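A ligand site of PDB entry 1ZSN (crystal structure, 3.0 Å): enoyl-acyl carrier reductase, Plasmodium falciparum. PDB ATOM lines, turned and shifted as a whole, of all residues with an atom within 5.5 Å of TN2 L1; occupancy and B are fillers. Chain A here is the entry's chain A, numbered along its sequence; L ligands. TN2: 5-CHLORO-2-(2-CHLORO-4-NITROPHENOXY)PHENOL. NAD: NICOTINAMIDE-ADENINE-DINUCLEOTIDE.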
ATOM      1  N   LEU A 120      21.414 -21.333  32.888  1.00  0.00           N
ATOM      2  CA  LEU A 120      20.172 -21.911  33.368  1.00  0.00           C
ATOM      3  C   LEU A 120      18.964 -21.423  32.615  1.00  0.00           C
ATOM      4  O   LEU A 120      18.946 -20.307  32.107  1.00  0.00           O
ATOM      5  CB  LEU A 120      20.012 -21.623  34.866  1.00  0.00           C
ATOM      6  CG  LEU A 120      19.767 -20.198  35.385  1.00  0.00           C
ATOM      7  CD1 LEU A 120      18.283 -19.965  35.529  1.00  0.00           C
ATOM      8  CD2 LEU A 120      20.466 -19.990  36.739  1.00  0.00           C
ATOM      9  N   ALA A 121      17.945 -22.280  32.535  1.00  0.00           N
ATOM     10  CA  ALA A 121      16.642 -21.912  31.975  1.00  0.00           C
ATOM     11  C   ALA A 121      15.526 -22.733  32.615  1.00  0.00           C
ATOM     12  O   ALA A 121      15.730 -23.870  33.070  1.00  0.00           O
ATOM     13  CB  ALA A 121      16.636 -22.088  30.462  1.00  0.00           C
ATOM     14  N   ASN A 122      14.343 -22.130  32.645  1.00  0.00           N
ATOM     15  CA  ASN A 122      13.121 -22.824  33.005  1.00  0.00           C
ATOM     16  C   ASN A 122      11.917 -22.220  32.295  1.00  0.00           C
ATOM     17  O   ASN A 122      11.767 -21.001  32.180  1.00  0.00           O
ATOM     18  CB  ASN A 122      12.915 -22.839  34.510  1.00  0.00           C
ATOM     19  CG  ASN A 122      12.361 -24.153  35.006  1.00  0.00           C
ATOM     20  OD1 ASN A 122      12.863 -24.707  35.990  1.00  0.00           O
ATOM     21  ND2 ASN A 122      11.319 -24.661  34.356  1.00  0.00           N
ATOM     22  N   ALA A 123      11.084 -23.099  31.781  1.00  0.00           N
ATOM     23  CA  ALA A 123       9.869 -22.724  31.119  1.00  0.00           C
ATOM     24  C   ALA A 123       8.813 -23.787  31.444  1.00  0.00           C
ATOM     25  O   ALA A 123       8.670 -24.789  30.715  1.00  0.00           O
ATOM     26  CB  ALA A 123      10.106 -22.629  29.619  1.00  0.00           C
ATOM     27  N   LYS A 124       8.092 -23.567  32.541  1.00  0.00           N
ATOM     28  CA  LYS A 124       6.998 -24.442  32.950  1.00  0.00           C
ATOM     29  C   LYS A 124       6.137 -24.981  31.804  1.00  0.00           C
ATOM     30  O   LYS A 124       5.726 -26.125  31.847  1.00  0.00           O
ATOM     31  CB  LYS A 124       6.085 -23.748  33.959  1.00  0.00           C
ATOM     32  CG  LYS A 124       6.637 -23.601  35.397  1.00  0.00           C
ATOM     33  CD  LYS A 124       5.673 -22.732  36.261  1.00  0.00           C
ATOM     34  CE  LYS A 124       5.996 -22.768  37.765  1.00  0.00           C
ATOM     35  NZ  LYS A 124       4.892 -22.120  38.570  1.00  0.00           N
ATOM     36  N   VAL A 126       7.007 -25.040  28.400  1.00  0.00           N
ATOM     37  CA  VAL A 126       7.766 -25.313  27.186  1.00  0.00           C
ATOM     38  C   VAL A 126       7.007 -26.216  26.193  1.00  0.00           C
ATOM     39  O   VAL A 126       7.060 -26.019  24.985  1.00  0.00           O
ATOM     40  CB  VAL A 126       9.193 -25.869  27.495  1.00  0.00           C
ATOM     41  CG1 VAL A 126       9.131 -27.201  28.245  1.00  0.00           C
ATOM     42  CG2 VAL A 126      10.008 -26.003  26.234  1.00  0.00           C
ATOM     43  N   THR A 170      22.600 -18.738  25.191  1.00  0.00           N
ATOM     44  CA  THR A 170      21.362 -18.429  24.505  1.00  0.00           C
ATOM     45  C   THR A 170      21.075 -19.485  23.431  1.00  0.00           C
ATOM     46  O   THR A 170      21.732 -20.535  23.403  1.00  0.00           O
ATOM     47  CB  THR A 170      21.357 -16.963  23.967  1.00  0.00           C
ATOM     48  OG1 THR A 170      20.035 -16.604  23.513  1.00  0.00           O
ATOM     49  CG2 THR A 170      22.357 -16.779  22.807  1.00  0.00           C
ATOM     50  N   TYR A 171      20.083 -19.228  22.576  1.00  0.00           N
ATOM     51  CA  TYR A 171      19.735 -20.169  21.520  1.00  0.00           C
ATOM     52  C   TYR A 171      18.976 -19.526  20.306  1.00  0.00           C
ATOM     53  O   TYR A 171      18.095 -18.658  20.455  1.00  0.00           O
ATOM     54  CB  TYR A 171      18.982 -21.365  22.132  1.00  0.00           C
ATOM     55  CG  TYR A 171      18.593 -22.420  21.144  1.00  0.00           C
ATOM     56  CD1 TYR A 171      19.553 -23.092  20.405  1.00  0.00           C
ATOM     57  CD2 TYR A 171      17.236 -22.753  20.949  1.00  0.00           C
ATOM     58  CE1 TYR A 171      19.192 -24.070  19.479  1.00  0.00           C
ATOM     59  CE2 TYR A 171      16.867 -23.737  20.027  1.00  0.00           C
ATOM     60  CZ  TYR A 171      17.857 -24.375  19.293  1.00  0.00           C
ATOM     61  OH  TYR A 171      17.532 -25.331  18.369  1.00  0.00           O
ATOM     62  N   TYR A 181      10.187 -25.489  20.510  1.00  0.00           N
ATOM     63  CA  TYR A 181      10.884 -24.711  21.532  1.00  0.00           C
ATOM     64  C   TYR A 181       9.949 -23.633  22.011  1.00  0.00           C
ATOM     65  O   TYR A 181      10.090 -22.466  21.637  1.00  0.00           O
ATOM     66  CB  TYR A 181      12.134 -24.073  20.921  1.00  0.00           C
ATOM     67  CG  TYR A 181      13.144 -23.524  21.885  1.00  0.00           C
ATOM     68  CD1 TYR A 181      13.993 -24.364  22.606  1.00  0.00           C
ATOM     69  CD2 TYR A 181      13.279 -22.156  22.048  1.00  0.00           C
ATOM     70  CE1 TYR A 181      14.947 -23.853  23.488  1.00  0.00           C
ATOM     71  CE2 TYR A 181      14.220 -21.628  22.932  1.00  0.00           C
ATOM     72  CZ  TYR A 181      15.040 -22.467  23.652  1.00  0.00           C
ATOM     73  OH  TYR A 181      15.962 -21.911  24.510  1.00  0.00           O
ATOM     74  N   MET A 185      10.303 -19.869  25.932  1.00  0.00           N
ATOM     75  CA  MET A 185      11.748 -20.020  25.757  1.00  0.00           C
ATOM     76  C   MET A 185      12.366 -19.161  24.651  1.00  0.00           C
ATOM     77  O   MET A 185      13.421 -18.569  24.855  1.00  0.00           O
ATOM     78  CB  MET A 185      12.143 -21.488  25.531  1.00  0.00           C
ATOM     79  CG  MET A 185      12.357 -22.280  26.798  1.00  0.00           C
ATOM     80  SD  MET A 185      13.254 -21.377  28.074  1.00  0.00           S
ATOM     81  CE  MET A 185      14.833 -21.070  27.267  1.00  0.00           C
ATOM     82  N   LYS A 189      14.945 -16.152  25.413  1.00  0.00           N
ATOM     83  CA  LYS A 189      16.283 -15.988  24.830  1.00  0.00           C
ATOM     84  C   LYS A 189      16.374 -14.698  24.001  1.00  0.00           C
ATOM     85  O   LYS A 189      17.419 -14.046  23.961  1.00  0.00           O
ATOM     86  CB  LYS A 189      16.667 -17.223  23.994  1.00  0.00           C
ATOM     87  CG  LYS A 189      16.633 -18.538  24.747  1.00  0.00           C
ATOM     88  CD  LYS A 189      17.414 -18.510  26.037  1.00  0.00           C
ATOM     89  CE  LYS A 189      18.174 -19.811  26.227  1.00  0.00           C
ATOM     90  NZ  LYS A 189      18.776 -19.962  27.582  1.00  0.00           N
ATOM     91  N   GLY A 217      24.785 -24.613  20.112  1.00  0.00           N
ATOM     92  CA  GLY A 217      24.007 -25.584  19.343  1.00  0.00           C
ATOM     93  C   GLY A 217      23.501 -26.666  20.272  1.00  0.00           C
ATOM     94  O   GLY A 217      23.547 -26.487  21.482  1.00  0.00           O
ATOM     95  N   PRO A 218      23.035 -27.792  19.733  1.00  0.00           N
ATOM     96  CA  PRO A 218      22.318 -28.677  20.636  1.00  0.00           C
ATOM     97  C   PRO A 218      23.246 -29.621  21.412  1.00  0.00           C
ATOM     98  O   PRO A 218      24.282 -30.100  20.890  1.00  0.00           O
ATOM     99  CB  PRO A 218      21.419 -29.462  19.704  1.00  0.00           C
ATOM    100  CG  PRO A 218      22.234 -29.583  18.437  1.00  0.00           C
ATOM    101  CD  PRO A 218      23.123 -28.356  18.373  1.00  0.00           C
ATOM    102  N   LEU A 219      22.872 -29.850  22.663  1.00  0.00           N
ATOM    103  CA  LEU A 219      23.526 -30.816  23.523  1.00  0.00           C
ATOM    104  C   LEU A 219      22.485 -31.622  24.279  1.00  0.00           C
ATOM    105  O   LEU A 219      21.508 -31.069  24.798  1.00  0.00           O
ATOM    106  CB  LEU A 219      24.435 -30.098  24.512  1.00  0.00           C
ATOM    107  CG  LEU A 219      25.348 -31.028  25.314  1.00  0.00           C
ATOM    108  CD1 LEU A 219      26.402 -31.652  24.395  1.00  0.00           C
ATOM    109  CD2 LEU A 219      25.992 -30.252  26.436  1.00  0.00           C
ATOM    110  N   SER A 221      21.533 -32.596  27.150  1.00  0.00           N
ATOM    111  CA  SER A 221      21.520 -32.411  28.603  1.00  0.00           C
ATOM    112  C   SER A 221      20.174 -32.818  29.174  1.00  0.00           C
ATOM    113  O   SER A 221      19.230 -33.080  28.425  1.00  0.00           O
ATOM    114  CB  SER A 221      21.821 -30.959  28.951  1.00  0.00           C
ATOM    115  OG  SER A 221      21.076 -30.074  28.142  1.00  0.00           O
ATOM    116  N   ALA A 223      17.981 -31.043  30.788  1.00  0.00           N
ATOM    117  CA  ALA A 223      16.988 -30.039  30.485  1.00  0.00           C
ATOM    118  C   ALA A 223      16.438 -30.264  29.098  1.00  0.00           C
ATOM    119  O   ALA A 223      15.233 -30.141  28.866  1.00  0.00           O
ATOM    120  CB  ALA A 223      17.577 -28.668  30.611  1.00  0.00           C
ATOM    121  N   ALA A 224      17.332 -30.601  28.165  1.00  0.00           N
ATOM    122  CA  ALA A 224      16.991 -30.747  26.753  1.00  0.00           C
ATOM    123  C   ALA A 224      16.149 -31.982  26.509  1.00  0.00           C
ATOM    124  O   ALA A 224      15.291 -31.974  25.613  1.00  0.00           O
ATOM    125  CB  ALA A 224      18.253 -30.790  25.926  1.00  0.00           C
ATOM    126  N   ILE A 227      12.406 -31.406  27.353  1.00  0.00           N
ATOM    127  CA  ILE A 227      11.495 -30.815  26.364  1.00  0.00           C
ATOM    128  C   ILE A 227      10.629 -31.923  25.741  1.00  0.00           C
ATOM    129  O   ILE A 227       9.398 -31.905  25.909  1.00  0.00           O
ATOM    130  CB  ILE A 227      12.223 -30.055  25.233  1.00  0.00           C
ATOM    131  CG1 ILE A 227      13.167 -29.001  25.806  1.00  0.00           C
ATOM    132  CG2 ILE A 227      11.191 -29.418  24.308  1.00  0.00           C
ATOM    133  CD1 ILE A 227      13.996 -28.303  24.764  1.00  0.00           C
ATOM    134  N   PHE A 272      12.646 -33.482  20.933  1.00  0.00           N
ATOM    135  CA  PHE A 272      13.051 -32.281  20.166  1.00  0.00           C
ATOM    136  C   PHE A 272      14.493 -31.868  20.435  1.00  0.00           C
ATOM    137  O   PHE A 272      14.822 -30.675  20.354  1.00  0.00           O
ATOM    138  CB  PHE A 272      12.134 -31.074  20.479  1.00  0.00           C
ATOM    139  CG  PHE A 272      10.697 -31.207  19.980  1.00  0.00           C
ATOM    140  CD1 PHE A 272      10.399 -31.878  18.789  1.00  0.00           C
ATOM    141  CD2 PHE A 272       9.643 -30.612  20.700  1.00  0.00           C
ATOM    142  CE1 PHE A 272       9.074 -31.976  18.341  1.00  0.00           C
ATOM    143  CE2 PHE A 272       8.318 -30.709  20.253  1.00  0.00           C
ATOM    144  CZ  PHE A 272       8.034 -31.389  19.078  1.00  0.00           C
ATOM    145  N   ILE A 273      15.329 -32.843  20.809  1.00  0.00           N
ATOM    146  CA  ILE A 273      16.775 -32.662  20.948  1.00  0.00           C
ATOM    147  C   ILE A 273      17.471 -33.707  20.100  1.00  0.00           C
ATOM    148  O   ILE A 273      18.528 -33.455  19.535  1.00  0.00           O
ATOM    149  CB  ILE A 273      17.274 -32.786  22.410  1.00  0.00           C
ATOM    150  CG1 ILE A 273      18.671 -32.195  22.554  1.00  0.00           C
ATOM    151  CG2 ILE A 273      17.304 -34.230  22.883  1.00  0.00           C
ATOM    152  CD1 ILE A 273      18.776 -30.707  22.309  1.00  0.00           C
ATOM    153  N   ALA A 276      17.251 -32.115  16.771  1.00  0.00           N
ATOM    154  CA  ALA A 276      18.217 -31.030  16.780  1.00  0.00           C
ATOM    155  C   ALA A 276      19.625 -31.545  16.508  1.00  0.00           C
ATOM    156  O   ALA A 276      20.292 -31.053  15.622  1.00  0.00           O
ATOM    157  CB  ALA A 276      18.158 -30.291  18.097  1.00  0.00           C
HETATM  158  O19 TN2 L   1      12.796 -25.028  31.098  1.00  0.00           O
HETATM  159  N17 TN2 L   1      12.884 -25.532  29.998  1.00  0.00           N
HETATM  160  O18 TN2 L   1      11.882 -25.991  29.482  1.00  0.00           O
HETATM  161  C14 TN2 L   1      14.119 -25.576  29.306  1.00  0.00           C
HETATM  162  C13 TN2 L   1      15.335 -25.490  30.003  1.00  0.00           C
HETATM  163  C11 TN2 L   1      16.536 -25.531  29.297  1.00  0.00           C
HETATM  164 CL12 TN2 L   1      18.145 -25.414  30.099  1.00  0.00          CL
HETATM  165  C15 TN2 L   1      14.118 -25.696  27.920  1.00  0.00           C
HETATM  166  C16 TN2 L   1      15.333 -25.729  27.233  1.00  0.00           C
HETATM  167  C10 TN2 L   1      16.541 -25.653  27.924  1.00  0.00           C
HETATM  168  O9  TN2 L   1      17.775 -25.678  27.301  1.00  0.00           O
HETATM  169  C6  TN2 L   1      17.881 -25.929  25.950  1.00  0.00           C
HETATM  170  C4  TN2 L   1      17.875 -24.875  25.037  1.00  0.00           C
HETATM  171  O5  TN2 L   1      17.773 -23.574  25.420  1.00  0.00           O
HETATM  172  C3  TN2 L   1      17.989 -25.141  23.672  1.00  0.00           C
HETATM  173  C7  TN2 L   1      17.985 -27.256  25.514  1.00  0.00           C
HETATM  174  C8  TN2 L   1      18.084 -27.522  24.148  1.00  0.00           C
HETATM  175  C2  TN2 L   1      18.085 -26.457  23.241  1.00  0.00           C
HETATM  176 CL20 TN2 L   1      18.226 -26.743  21.494  1.00  0.00          CL
HETATM  177  PA  NAD L   2      20.979 -28.182  32.103  1.00  0.00           P
HETATM  178  O1A NAD L   2      19.914 -29.070  32.665  1.00  0.00           O
HETATM  179  O2A NAD L   2      22.435 -28.571  32.183  1.00  0.00           O
HETATM  180  O5B NAD L   2      20.862 -26.751  32.823  1.00  0.00           O
HETATM  181  C5B NAD L   2      19.622 -26.188  33.175  1.00  0.00           C
HETATM  182  C4B NAD L   2      19.710 -25.928  34.659  1.00  0.00           C
HETATM  183  O4B NAD L   2      18.805 -24.902  35.008  1.00  0.00           O
HETATM  184  C3B NAD L   2      19.246 -27.099  35.511  1.00  0.00           C
HETATM  185  O3B NAD L   2      20.316 -28.013  35.747  1.00  0.00           O
HETATM  186  C2B NAD L   2      18.795 -26.451  36.810  1.00  0.00           C
HETATM  187  O2B NAD L   2      19.876 -26.491  37.760  1.00  0.00           O
HETATM  188  C1B NAD L   2      18.663 -25.005  36.424  1.00  0.00           C
HETATM  189  N9A NAD L   2      17.446 -24.301  36.885  1.00  0.00           N
HETATM  190  C8A NAD L   2      16.210 -24.396  36.326  1.00  0.00           C
HETATM  191  N7A NAD L   2      15.337 -23.570  36.989  1.00  0.00           N
HETATM  192  C5A NAD L   2      16.015 -22.946  37.987  1.00  0.00           C
HETATM  193  C6A NAD L   2      15.693 -22.014  38.967  1.00  0.00           C
HETATM  194  N6A NAD L   2      14.410 -21.557  39.058  1.00  0.00           N
HETATM  195  N1A NAD L   2      16.687 -21.599  39.819  1.00  0.00           N
HETATM  196  C2A NAD L   2      17.963 -22.045  39.734  1.00  0.00           C
HETATM  197  N3A NAD L   2      18.335 -22.950  38.797  1.00  0.00           N
HETATM  198  C4A NAD L   2      17.417 -23.426  37.910  1.00  0.00           C
HETATM  199  O3  NAD L   2      20.630 -27.931  30.535  1.00  0.00           O
HETATM  200  PN  NAD L   2      21.529 -27.062  29.509  1.00  0.00           P
HETATM  201  O1N NAD L   2      20.867 -27.180  28.166  1.00  0.00           O
HETATM  202  O2N NAD L   2      22.984 -27.411  29.636  1.00  0.00           O
HETATM  203  O5D NAD L   2      21.270 -25.576  30.086  1.00  0.00           O
HETATM  204  C5D NAD L   2      22.286 -24.585  30.166  1.00  0.00           C
HETATM  205  C4D NAD L   2      21.988 -23.383  29.262  1.00  0.00           C
HETATM  206  O4D NAD L   2      22.363 -23.669  27.901  1.00  0.00           O
HETATM  207  C3D NAD L   2      20.506 -23.062  29.249  1.00  0.00           C
HETATM  208  O3D NAD L   2      20.284 -21.660  29.332  1.00  0.00           O
HETATM  209  C2D NAD L   2      20.052 -23.540  27.891  1.00  0.00           C
HETATM  210  O2D NAD L   2      18.910 -22.770  27.546  1.00  0.00           O
HETATM  211  C1D NAD L   2      21.291 -23.247  27.050  1.00  0.00           C
HETATM  212  N1N NAD L   2      21.335 -23.962  25.777  1.00  0.00           N
HETATM  213  C2N NAD L   2      21.345 -25.317  25.733  1.00  0.00           C
HETATM  214  C3N NAD L   2      21.387 -26.018  24.519  1.00  0.00           C
HETATM  215  C7N NAD L   2      21.357 -27.527  24.463  1.00  0.00           C
HETATM  216  O7N NAD L   2      21.125 -28.113  23.308  1.00  0.00           O
HETATM  217  N7N NAD L   2      21.504 -28.262  25.476  1.00  0.00           N
HETATM  218  C4N NAD L   2      21.423 -25.271  23.347  1.00  0.00           C
HETATM  219  C5N NAD L   2      21.428 -23.874  23.414  1.00  0.00           C
HETATM  220  C6N NAD L   2      21.383 -23.240  24.651  1.00  0.00           C
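An oxygen (O2D) of NAD L2 is in hydrogen-bond range of an oxygen (O5) of TN2 L1 (2.5 Å).
O of Leu 219 is in hydrogen-bond range of N7N of NAD L2, 2.9 Å away. The backbone carbonyl oxygen (O) of Leu 120 is in hydrogen-bond range of an oxygen (O3D) of NAD L2. OG of Ser 221 is in hydrogen-bond range of O1N of NAD L2. The side-chain hydroxyl of Tyr 181 sits at hydrogen-bond distance from an oxygen (O5) of TN2 L1 (2.6 Å). An oxygen (O2D) of NAD L2 sits at hydrogen-bond distance from the side-chain amino group (NZ) of Lys 189. The backbone NH (N) of Ala 123 is in hydrogen-bond range of an oxygen (O19) of TN2 L1 (2.7 Å). N of Leu 219 sits at hydrogen-bond distance from O7N of NAD L2 (2.5 Å). N of Ala 223 sits close to O1A of NAD L2, at 3.3 Å. N7A of NAD L2 lies close to OD1 of Asn 122 (2.9 Å).
Merely in contact with TN2 L1: Asn 122 (2.9 Å), Val 126 (3.2 Å), Tyr 171 (3.3 Å), Ala 223 (3.3 Å), Ala 121 (3.5 Å), Ala 224 (3.6 Å), Ile 273 (3.7 Å), Ile 227 (3.8 Å) and Lys 189 (3.9 Å). Of the 21 residues printed, 11 come within 4 Å of TN2 L1. The nearest printed residue that does not touch TN2 L1 is Met 185 (4.004 Å).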
